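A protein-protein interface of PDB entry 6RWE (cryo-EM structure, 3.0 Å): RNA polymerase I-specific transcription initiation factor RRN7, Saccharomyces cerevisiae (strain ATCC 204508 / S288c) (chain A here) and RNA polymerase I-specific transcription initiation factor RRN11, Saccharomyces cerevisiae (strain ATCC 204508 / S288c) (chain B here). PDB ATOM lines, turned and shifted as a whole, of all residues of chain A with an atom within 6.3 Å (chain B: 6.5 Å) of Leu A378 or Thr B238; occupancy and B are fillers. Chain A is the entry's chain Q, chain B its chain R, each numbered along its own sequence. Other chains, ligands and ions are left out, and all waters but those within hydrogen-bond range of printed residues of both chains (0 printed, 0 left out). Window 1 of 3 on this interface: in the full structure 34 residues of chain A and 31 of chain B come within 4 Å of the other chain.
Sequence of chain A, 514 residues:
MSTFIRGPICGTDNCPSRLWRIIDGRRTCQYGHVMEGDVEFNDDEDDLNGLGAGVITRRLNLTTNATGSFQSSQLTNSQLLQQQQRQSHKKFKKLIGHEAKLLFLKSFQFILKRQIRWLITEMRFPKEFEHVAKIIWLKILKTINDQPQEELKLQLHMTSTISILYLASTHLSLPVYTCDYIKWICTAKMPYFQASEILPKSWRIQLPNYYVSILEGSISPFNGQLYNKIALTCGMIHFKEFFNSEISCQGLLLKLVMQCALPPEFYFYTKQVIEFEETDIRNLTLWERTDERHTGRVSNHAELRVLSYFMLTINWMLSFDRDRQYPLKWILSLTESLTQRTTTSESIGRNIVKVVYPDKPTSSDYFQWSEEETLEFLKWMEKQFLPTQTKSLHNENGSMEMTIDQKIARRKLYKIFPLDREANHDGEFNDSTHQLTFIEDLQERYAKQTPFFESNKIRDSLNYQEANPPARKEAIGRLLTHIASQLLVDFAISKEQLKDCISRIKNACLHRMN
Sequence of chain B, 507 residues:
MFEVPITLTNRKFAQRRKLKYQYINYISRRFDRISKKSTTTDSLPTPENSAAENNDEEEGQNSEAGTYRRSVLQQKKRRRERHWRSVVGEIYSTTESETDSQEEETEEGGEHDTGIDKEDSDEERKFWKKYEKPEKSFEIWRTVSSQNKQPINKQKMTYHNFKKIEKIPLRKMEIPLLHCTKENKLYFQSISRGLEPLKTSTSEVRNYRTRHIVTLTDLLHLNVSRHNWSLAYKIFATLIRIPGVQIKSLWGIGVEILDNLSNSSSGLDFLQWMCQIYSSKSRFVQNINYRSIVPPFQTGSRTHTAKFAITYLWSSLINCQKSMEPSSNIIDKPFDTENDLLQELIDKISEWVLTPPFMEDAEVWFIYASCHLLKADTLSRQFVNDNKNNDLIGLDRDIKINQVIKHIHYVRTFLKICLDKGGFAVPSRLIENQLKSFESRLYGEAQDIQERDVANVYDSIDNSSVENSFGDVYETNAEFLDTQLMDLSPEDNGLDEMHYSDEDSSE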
ATOM      1  N   GLU A 373       3.384  16.378 -20.173  1.00  0.00           N
ATOM      2  CA  GLU A 373       4.432  15.746 -19.383  1.00  0.00           C
ATOM      3  C   GLU A 373       4.056  15.672 -17.909  1.00  0.00           C
ATOM      4  O   GLU A 373       4.573  14.816 -17.185  1.00  0.00           O
ATOM      5  CB  GLU A 373       5.742  16.508 -19.589  1.00  0.00           C
ATOM      6  CG  GLU A 373       6.996  15.849 -19.040  1.00  0.00           C
ATOM      7  CD  GLU A 373       8.255  16.581 -19.446  1.00  0.00           C
ATOM      8  OE1 GLU A 373       8.145  17.617 -20.134  1.00  0.00           O
ATOM      9  OE2 GLU A 373       9.355  16.114 -19.092  1.00  0.00           O
ATOM     10  N   THR A 374       3.134  16.518 -17.462  1.00  0.00           N
ATOM     11  CA  THR A 374       2.668  16.459 -16.085  1.00  0.00           C
ATOM     12  C   THR A 374       1.669  15.327 -15.881  1.00  0.00           C
ATOM     13  O   THR A 374       1.689  14.668 -14.835  1.00  0.00           O
ATOM     14  CB  THR A 374       2.054  17.804 -15.703  1.00  0.00           C
ATOM     15  OG1 THR A 374       3.006  18.841 -15.961  1.00  0.00           O
ATOM     16  CG2 THR A 374       1.693  17.842 -14.235  1.00  0.00           C
ATOM     17  N   LEU A 375       0.802  15.076 -16.873  1.00  0.00           N
ATOM     18  CA  LEU A 375      -0.219  14.036 -16.736  1.00  0.00           C
ATOM     19  C   LEU A 375       0.397  12.650 -16.626  1.00  0.00           C
ATOM     20  O   LEU A 375      -0.075  11.817 -15.845  1.00  0.00           O
ATOM     21  CB  LEU A 375      -1.193  14.060 -17.913  1.00  0.00           C
ATOM     22  CG  LEU A 375      -2.397  15.000 -17.942  1.00  0.00           C
ATOM     23  CD1 LEU A 375      -2.002  16.396 -18.331  1.00  0.00           C
ATOM     24  CD2 LEU A 375      -3.468  14.467 -18.873  1.00  0.00           C
ATOM     25  N   GLU A 376       1.457  12.390 -17.386  1.00  0.00           N
ATOM     26  CA  GLU A 376       2.084  11.079 -17.342  1.00  0.00           C
ATOM     27  C   GLU A 376       2.895  10.885 -16.070  1.00  0.00           C
ATOM     28  O   GLU A 376       3.083   9.744 -15.634  1.00  0.00           O
ATOM     29  CB  GLU A 376       2.952  10.879 -18.588  1.00  0.00           C
ATOM     30  CG  GLU A 376       3.445   9.454 -18.817  1.00  0.00           C
ATOM     31  CD  GLU A 376       2.324   8.478 -19.142  1.00  0.00           C
ATOM     32  OE1 GLU A 376       1.283   8.907 -19.687  1.00  0.00           O
ATOM     33  OE2 GLU A 376       2.489   7.273 -18.852  1.00  0.00           O
ATOM     34  N   PHE A 377       3.359  11.978 -15.459  1.00  0.00           N
ATOM     35  CA  PHE A 377       3.884  11.904 -14.103  1.00  0.00           C
ATOM     36  C   PHE A 377       2.810  11.431 -13.138  1.00  0.00           C
ATOM     37  O   PHE A 377       3.078  10.615 -12.251  1.00  0.00           O
ATOM     38  CB  PHE A 377       4.417  13.269 -13.677  1.00  0.00           C
ATOM     39  CG  PHE A 377       4.981  13.305 -12.285  1.00  0.00           C
ATOM     40  CD1 PHE A 377       6.248  12.831 -12.028  1.00  0.00           C
ATOM     41  CD2 PHE A 377       4.248  13.831 -11.236  1.00  0.00           C
ATOM     42  CE1 PHE A 377       6.778  12.873 -10.753  1.00  0.00           C
ATOM     43  CE2 PHE A 377       4.772  13.870  -9.959  1.00  0.00           C
ATOM     44  CZ  PHE A 377       6.038  13.390  -9.719  1.00  0.00           C
ATOM     45  N   LEU A 378       1.586  11.917 -13.307  1.00  0.00           N
ATOM     46  CA  LEU A 378       0.513  11.522 -12.410  1.00  0.00           C
ATOM     47  C   LEU A 378      -0.005  10.130 -12.718  1.00  0.00           C
ATOM     48  O   LEU A 378      -0.595   9.492 -11.841  1.00  0.00           O
ATOM     49  CB  LEU A 378      -0.619  12.544 -12.477  1.00  0.00           C
ATOM     50  CG  LEU A 378      -0.156  13.930 -12.029  1.00  0.00           C
ATOM     51  CD1 LEU A 378      -1.259  14.940 -12.200  1.00  0.00           C
ATOM     52  CD2 LEU A 378       0.330  13.899 -10.599  1.00  0.00           C
ATOM     53  N   LYS A 379       0.207   9.642 -13.936  1.00  0.00           N
ATOM     54  CA  LYS A 379      -0.064   8.244 -14.217  1.00  0.00           C
ATOM     55  C   LYS A 379       1.049   7.348 -13.709  1.00  0.00           C
ATOM     56  O   LYS A 379       0.811   6.164 -13.455  1.00  0.00           O
ATOM     57  CB  LYS A 379      -0.267   8.043 -15.715  1.00  0.00           C
ATOM     58  CG  LYS A 379      -1.501   8.745 -16.235  1.00  0.00           C
ATOM     59  CD  LYS A 379      -1.624   8.614 -17.735  1.00  0.00           C
ATOM     60  CE  LYS A 379      -2.016   7.202 -18.116  1.00  0.00           C
ATOM     61  NZ  LYS A 379      -2.280   7.088 -19.572  1.00  0.00           N
ATOM     62  N   TRP A 380       2.255   7.894 -13.546  1.00  0.00           N
ATOM     63  CA  TRP A 380       3.292   7.176 -12.823  1.00  0.00           C
ATOM     64  C   TRP A 380       2.978   7.105 -11.338  1.00  0.00           C
ATOM     65  O   TRP A 380       3.390   6.156 -10.663  1.00  0.00           O
ATOM     66  CB  TRP A 380       4.650   7.839 -13.031  1.00  0.00           C
ATOM     67  CG  TRP A 380       5.718   7.181 -12.245  1.00  0.00           C
ATOM     68  CD1 TRP A 380       6.284   5.973 -12.490  1.00  0.00           C
ATOM     69  CD2 TRP A 380       6.270   7.642 -11.012  1.00  0.00           C
ATOM     70  NE1 TRP A 380       7.202   5.675 -11.516  1.00  0.00           N
ATOM     71  CE2 TRP A 380       7.207   6.685 -10.592  1.00  0.00           C
ATOM     72  CE3 TRP A 380       6.078   8.782 -10.234  1.00  0.00           C
ATOM     73  CZ2 TRP A 380       7.952   6.833  -9.428  1.00  0.00           C
ATOM     74  CZ3 TRP A 380       6.821   8.929  -9.082  1.00  0.00           C
ATOM     75  CH2 TRP A 380       7.747   7.960  -8.690  1.00  0.00           C
ATOM     76  N   MET A 381       2.222   8.078 -10.821  1.00  0.00           N
ATOM     77  CA  MET A 381       1.888   8.112  -9.400  1.00  0.00           C
ATOM     78  C   MET A 381       1.014   6.946  -8.963  1.00  0.00           C
ATOM     79  O   MET A 381       0.988   6.630  -7.773  1.00  0.00           O
ATOM     80  CB  MET A 381       1.213   9.430  -9.051  1.00  0.00           C
ATOM     81  CG  MET A 381       2.154  10.609  -9.071  1.00  0.00           C
ATOM     82  SD  MET A 381       3.499  10.367  -7.904  1.00  0.00           S
ATOM     83  CE  MET A 381       2.591  10.384  -6.370  1.00  0.00           C
ATOM     84  N   GLU A 382       0.349   6.264  -9.895  1.00  0.00           N
ATOM     85  CA  GLU A 382      -0.283   4.979  -9.623  1.00  0.00           C
ATOM     86  C   GLU A 382       0.705   3.807  -9.687  1.00  0.00           C
ATOM     87  O   GLU A 382       0.289   2.661  -9.885  1.00  0.00           O
ATOM     88  CB  GLU A 382      -1.429   4.739 -10.605  1.00  0.00           C
ATOM     89  CG  GLU A 382      -2.564   5.733 -10.506  1.00  0.00           C
ATOM     90  CD  GLU A 382      -3.619   5.479 -11.555  1.00  0.00           C
ATOM     91  OE1 GLU A 382      -3.412   4.572 -12.386  1.00  0.00           O
ATOM     92  OE2 GLU A 382      -4.641   6.189 -11.570  1.00  0.00           O
ATOM     93  N   PHE A 385       2.020   4.501  -4.897  1.00  0.00           N
ATOM     94  CA  PHE A 385       1.220   4.106  -3.739  1.00  0.00           C
ATOM     95  C   PHE A 385       1.211   2.602  -3.544  1.00  0.00           C
ATOM     96  O   PHE A 385       1.128   2.125  -2.409  1.00  0.00           O
ATOM     97  CB  PHE A 385      -0.225   4.560  -3.886  1.00  0.00           C
ATOM     98  CG  PHE A 385      -0.384   6.018  -4.094  1.00  0.00           C
ATOM     99  CD1 PHE A 385      -0.094   6.909  -3.084  1.00  0.00           C
ATOM    100  CD2 PHE A 385      -0.900   6.494  -5.280  1.00  0.00           C
ATOM    101  CE1 PHE A 385      -0.264   8.255  -3.281  1.00  0.00           C
ATOM    102  CE2 PHE A 385      -1.072   7.833  -5.481  1.00  0.00           C
ATOM    103  CZ  PHE A 385      -0.756   8.716  -4.481  1.00  0.00           C
ATOM    104  N   LEU A 419      -9.809   8.872  -7.228  1.00  0.00           N
ATOM    105  CA  LEU A 419      -8.446   9.048  -7.715  1.00  0.00           C
ATOM    106  C   LEU A 419      -8.384   9.187  -9.225  1.00  0.00           C
ATOM    107  O   LEU A 419      -7.471   9.841  -9.735  1.00  0.00           O
ATOM    108  CB  LEU A 419      -7.588   7.875  -7.229  1.00  0.00           C
ATOM    109  CG  LEU A 419      -6.060   7.842  -7.321  1.00  0.00           C
ATOM    110  CD1 LEU A 419      -5.551   7.302  -8.625  1.00  0.00           C
ATOM    111  CD2 LEU A 419      -5.516   9.233  -7.112  1.00  0.00           C
ATOM    112  N   LEU B 216       5.057  17.696  -5.500  1.00  0.00           N
ATOM    113  CA  LEU B 216       3.623  17.718  -5.740  1.00  0.00           C
ATOM    114  C   LEU B 216       2.900  18.880  -5.080  1.00  0.00           C
ATOM    115  O   LEU B 216       1.748  19.137  -5.435  1.00  0.00           O
ATOM    116  CB  LEU B 216       2.978  16.421  -5.275  1.00  0.00           C
ATOM    117  CG  LEU B 216       3.199  15.213  -6.160  1.00  0.00           C
ATOM    118  CD1 LEU B 216       2.649  14.013  -5.462  1.00  0.00           C
ATOM    119  CD2 LEU B 216       2.483  15.436  -7.458  1.00  0.00           C
ATOM    120  N   LEU B 219       3.951  21.838  -7.569  1.00  0.00           N
ATOM    121  CA  LEU B 219       3.134  21.685  -8.762  1.00  0.00           C
ATOM    122  C   LEU B 219       1.662  21.914  -8.485  1.00  0.00           C
ATOM    123  O   LEU B 219       0.906  22.172  -9.425  1.00  0.00           O
ATOM    124  CB  LEU B 219       3.300  20.297  -9.372  1.00  0.00           C
ATOM    125  CG  LEU B 219       4.635  19.963 -10.017  1.00  0.00           C
ATOM    126  CD1 LEU B 219       4.633  18.525 -10.478  1.00  0.00           C
ATOM    127  CD2 LEU B 219       4.880  20.892 -11.175  1.00  0.00           C
ATOM    128  N   LEU B 231      -6.289  19.579 -14.273  1.00  0.00           N
ATOM    129  CA  LEU B 231      -5.004  18.991 -13.928  1.00  0.00           C
ATOM    130  C   LEU B 231      -4.679  19.144 -12.452  1.00  0.00           C
ATOM    131  O   LEU B 231      -4.135  18.215 -11.847  1.00  0.00           O
ATOM    132  CB  LEU B 231      -3.897  19.616 -14.780  1.00  0.00           C
ATOM    133  CG  LEU B 231      -2.484  19.087 -14.552  1.00  0.00           C
ATOM    134  CD1 LEU B 231      -2.453  17.595 -14.789  1.00  0.00           C
ATOM    135  CD2 LEU B 231      -1.499  19.776 -15.464  1.00  0.00           C
ATOM    136  N   TYR B 233      -6.829  19.163 -10.105  1.00  0.00           N
ATOM    137  CA  TYR B 233      -7.628  18.154  -9.427  1.00  0.00           C
ATOM    138  C   TYR B 233      -6.905  16.820  -9.374  1.00  0.00           C
ATOM    139  O   TYR B 233      -7.033  16.089  -8.388  1.00  0.00           O
ATOM    140  CB  TYR B 233      -8.972  17.992 -10.127  1.00  0.00           C
ATOM    141  CG  TYR B 233      -9.841  16.905  -9.547  1.00  0.00           C
ATOM    142  CD1 TYR B 233     -10.511  17.090  -8.353  1.00  0.00           C
ATOM    143  CD2 TYR B 233      -9.996  15.693 -10.203  1.00  0.00           C
ATOM    144  CE1 TYR B 233     -11.305  16.103  -7.827  1.00  0.00           C
ATOM    145  CE2 TYR B 233     -10.785  14.699  -9.682  1.00  0.00           C
ATOM    146  CZ  TYR B 233     -11.437  14.909  -8.495  1.00  0.00           C
ATOM    147  OH  TYR B 233     -12.228  13.918  -7.977  1.00  0.00           O
ATOM    148  N   LYS B 234      -6.153  16.482 -10.419  1.00  0.00           N
ATOM    149  CA  LYS B 234      -5.433  15.217 -10.417  1.00  0.00           C
ATOM    150  C   LYS B 234      -4.240  15.251  -9.484  1.00  0.00           C
ATOM    151  O   LYS B 234      -3.834  14.206  -8.969  1.00  0.00           O
ATOM    152  CB  LYS B 234      -4.974  14.861 -11.823  1.00  0.00           C
ATOM    153  CG  LYS B 234      -6.081  14.439 -12.752  1.00  0.00           C
ATOM    154  CD  LYS B 234      -5.503  14.039 -14.094  1.00  0.00           C
ATOM    155  CE  LYS B 234      -6.594  13.654 -15.060  1.00  0.00           C
ATOM    156  NZ  LYS B 234      -7.228  12.397 -14.603  1.00  0.00           N
ATOM    157  N   ILE B 235      -3.659  16.428  -9.261  1.00  0.00           N
ATOM    158  CA  ILE B 235      -2.518  16.518  -8.361  1.00  0.00           C
ATOM    159  C   ILE B 235      -2.974  16.377  -6.924  1.00  0.00           C
ATOM    160  O   ILE B 235      -2.372  15.645  -6.135  1.00  0.00           O
ATOM    161  CB  ILE B 235      -1.771  17.839  -8.581  1.00  0.00           C
ATOM    162  CG1 ILE B 235      -1.329  17.950 -10.029  1.00  0.00           C
ATOM    163  CG2 ILE B 235      -0.554  17.914  -7.682  1.00  0.00           C
ATOM    164  CD1 ILE B 235      -0.863  19.305 -10.397  1.00  0.00           C
ATOM    165  N   PHE B 236      -4.057  17.059  -6.566  1.00  0.00           N
ATOM    166  CA  PHE B 236      -4.522  17.040  -5.190  1.00  0.00           C
ATOM    167  C   PHE B 236      -5.183  15.724  -4.829  1.00  0.00           C
ATOM    168  O   PHE B 236      -5.214  15.366  -3.649  1.00  0.00           O
ATOM    169  CB  PHE B 236      -5.470  18.211  -4.969  1.00  0.00           C
ATOM    170  CG  PHE B 236      -5.926  18.358  -3.563  1.00  0.00           C
ATOM    171  CD1 PHE B 236      -5.017  18.637  -2.564  1.00  0.00           C
ATOM    172  CD2 PHE B 236      -7.260  18.275  -3.244  1.00  0.00           C
ATOM    173  CE1 PHE B 236      -5.430  18.797  -1.271  1.00  0.00           C
ATOM    174  CE2 PHE B 236      -7.671  18.435  -1.952  1.00  0.00           C
ATOM    175  CZ  PHE B 236      -6.758  18.691  -0.969  1.00  0.00           C
ATOM    176  N   ALA B 237      -5.686  14.983  -5.815  1.00  0.00           N
ATOM    177  CA  ALA B 237      -6.192  13.648  -5.537  1.00  0.00           C
ATOM    178  C   ALA B 237      -5.060  12.695  -5.185  1.00  0.00           C
ATOM    179  O   ALA B 237      -5.217  11.832  -4.318  1.00  0.00           O
ATOM    180  CB  ALA B 237      -6.982  13.123  -6.731  1.00  0.00           C
ATOM    181  N   THR B 238      -3.910  12.838  -5.836  1.00  0.00           N
ATOM    182  CA  THR B 238      -2.757  12.014  -5.516  1.00  0.00           C
ATOM    183  C   THR B 238      -1.947  12.558  -4.357  1.00  0.00           C
ATOM    184  O   THR B 238      -1.080  11.849  -3.842  1.00  0.00           O
ATOM    185  CB  THR B 238      -1.821  11.886  -6.714  1.00  0.00           C
ATOM    186  OG1 THR B 238      -1.289  13.173  -7.034  1.00  0.00           O
ATOM    187  CG2 THR B 238      -2.556  11.340  -7.912  1.00  0.00           C
ATOM    188  N   LEU B 239      -2.177  13.796  -3.955  1.00  0.00           N
ATOM    189  CA  LEU B 239      -1.390  14.352  -2.870  1.00  0.00           C
ATOM    190  C   LEU B 239      -1.933  13.948  -1.516  1.00  0.00           C
ATOM    191  O   LEU B 239      -1.154  13.687  -0.596  1.00  0.00           O
ATOM    192  CB  LEU B 239      -1.340  15.874  -2.990  1.00  0.00           C
ATOM    193  CG  LEU B 239      -0.456  16.582  -1.975  1.00  0.00           C
ATOM    194  CD1 LEU B 239       0.955  16.087  -2.117  1.00  0.00           C
ATOM    195  CD2 LEU B 239      -0.512  18.064  -2.185  1.00  0.00           C
ATOM    196  N   ILE B 240      -3.256  13.837  -1.387  1.00  0.00           N
ATOM    197  CA  ILE B 240      -3.868  13.464  -0.117  1.00  0.00           C
ATOM    198  C   ILE B 240      -3.718  11.993   0.216  1.00  0.00           C
ATOM    199  O   ILE B 240      -4.074  11.582   1.326  1.00  0.00           O
ATOM    200  CB  ILE B 240      -5.360  13.824  -0.133  1.00  0.00           C
ATOM    201  CG1 ILE B 240      -6.042  13.113  -1.292  1.00  0.00           C
ATOM    202  CG2 ILE B 240      -5.524  15.305  -0.268  1.00  0.00           C
ATOM    203  CD1 ILE B 240      -7.528  13.230  -1.282  1.00  0.00           C
ATOM    204  N   ARG B 241      -3.202  11.188  -0.707  1.00  0.00           N
ATOM    205  CA  ARG B 241      -3.044   9.761  -0.499  1.00  0.00           C
ATOM    206  C   ARG B 241      -1.637   9.365  -0.080  1.00  0.00           C
ATOM    207  O   ARG B 241      -1.436   8.221   0.333  1.00  0.00           O
ATOM    208  CB  ARG B 241      -3.447   9.015  -1.769  1.00  0.00           C
ATOM    209  CG  ARG B 241      -4.940   9.032  -2.005  1.00  0.00           C
ATOM    210  CD  ARG B 241      -5.312   8.393  -3.312  1.00  0.00           C
ATOM    211  NE  ARG B 241      -6.751   8.236  -3.459  1.00  0.00           N
ATOM    212  CZ  ARG B 241      -7.565   9.168  -3.934  1.00  0.00           C
ATOM    213  NH1 ARG B 241      -8.861   8.928  -4.043  1.00  0.00           N
ATOM    214  NH2 ARG B 241      -7.089  10.346  -4.289  1.00  0.00           N
ATOM    215  N   ILE B 242      -0.672  10.265  -0.165  1.00  0.00           N
ATOM    216  CA  ILE B 242       0.674   9.959   0.328  1.00  0.00           C
ATOM    217  C   ILE B 242       0.661  10.001   1.850  1.00  0.00           C
ATOM    218  O   ILE B 242       0.100  10.943   2.431  1.00  0.00           O
ATOM    219  CB  ILE B 242       1.685  10.949  -0.251  1.00  0.00           C
ATOM    220  CG1 ILE B 242       1.807  10.745  -1.753  1.00  0.00           C
ATOM    221  CG2 ILE B 242       3.047  10.803   0.387  1.00  0.00           C
ATOM    222  CD1 ILE B 242       2.617  11.790  -2.432  1.00  0.00           C
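Hydrophobic or aromatic side chains of chain A that line the printed part of chain B: Leu A375, Phe A377, Leu A378, Met A381, Phe A385 and Leu A419.
Of the 13 printed residues of chain B, 8 touch a printed residue of chain A.
Hydrophobic or aromatic side chains of chain B that line the printed part of chain A: Leu B216, Leu B231, Ile B235 and Ile B242.
Among the printed residues, 14 pairs touch across the chains.
Among the printed residues, no Asp or Glu carboxylate lies within 4 Å of a Lys or Arg side-chain nitrogen of the other chain.
O of Ile B235 is in hydrogen-bond range of OG1 of Thr B238 (2.8 Å).
O of Lys B234 sits close to OG1 of Thr B238, 3.4 Å away.
The backbone NH (N) of Leu A419 sits close to the guanidinium group (NH1) of Arg B241 (3.3 Å).
Glu A376 touches none of the printed residues of chain B.
Of the printed residues of chain B, Leu A378 touches Leu B231 (3.9 Å), Lys B234 (3.7 Å), Ile B235 (3.7 Å) and Thr B238 (3.98 Å).
Of the printed residues of chain A, Leu B216 touches Phe A377 (3.7 Å) and Met A381 (3.7 Å).
Of the printed residues of chain A, Ile B235 touches Leu A378.
Of the printed residues of chain A, Thr B238 touches Leu A378 (3.98 Å), Phe A385 (3.2 Å) and Leu A419 (3.7 Å).
Of the printed residues of chain A, Arg B241 touches Phe A385 and Leu A419.
The nearest printed residue of chain B that does not touch Phe A377 is Leu B219 (4.7 Å).
Leu A375 touches Leu B231.
Phe A377 touches Leu B216.
Leu A378 touches Leu B231.
Leu A378 touches Lys B234 (CD1 to CB, 3.7 Å).
Ile B235 touches Leu A378 (CG1 to CD1, 3.7 Å).
Leu A378 touches Thr B238.
CE of Met A381 touches CD1 of Leu B216, 3.7 Å away.
Thr B238 touches Phe A385 (O to CZ, 3.2 Å).
Phe A385 touches Arg B241.
CD2 of Leu A419 touches O of Ala B237, 3.8 Å away.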
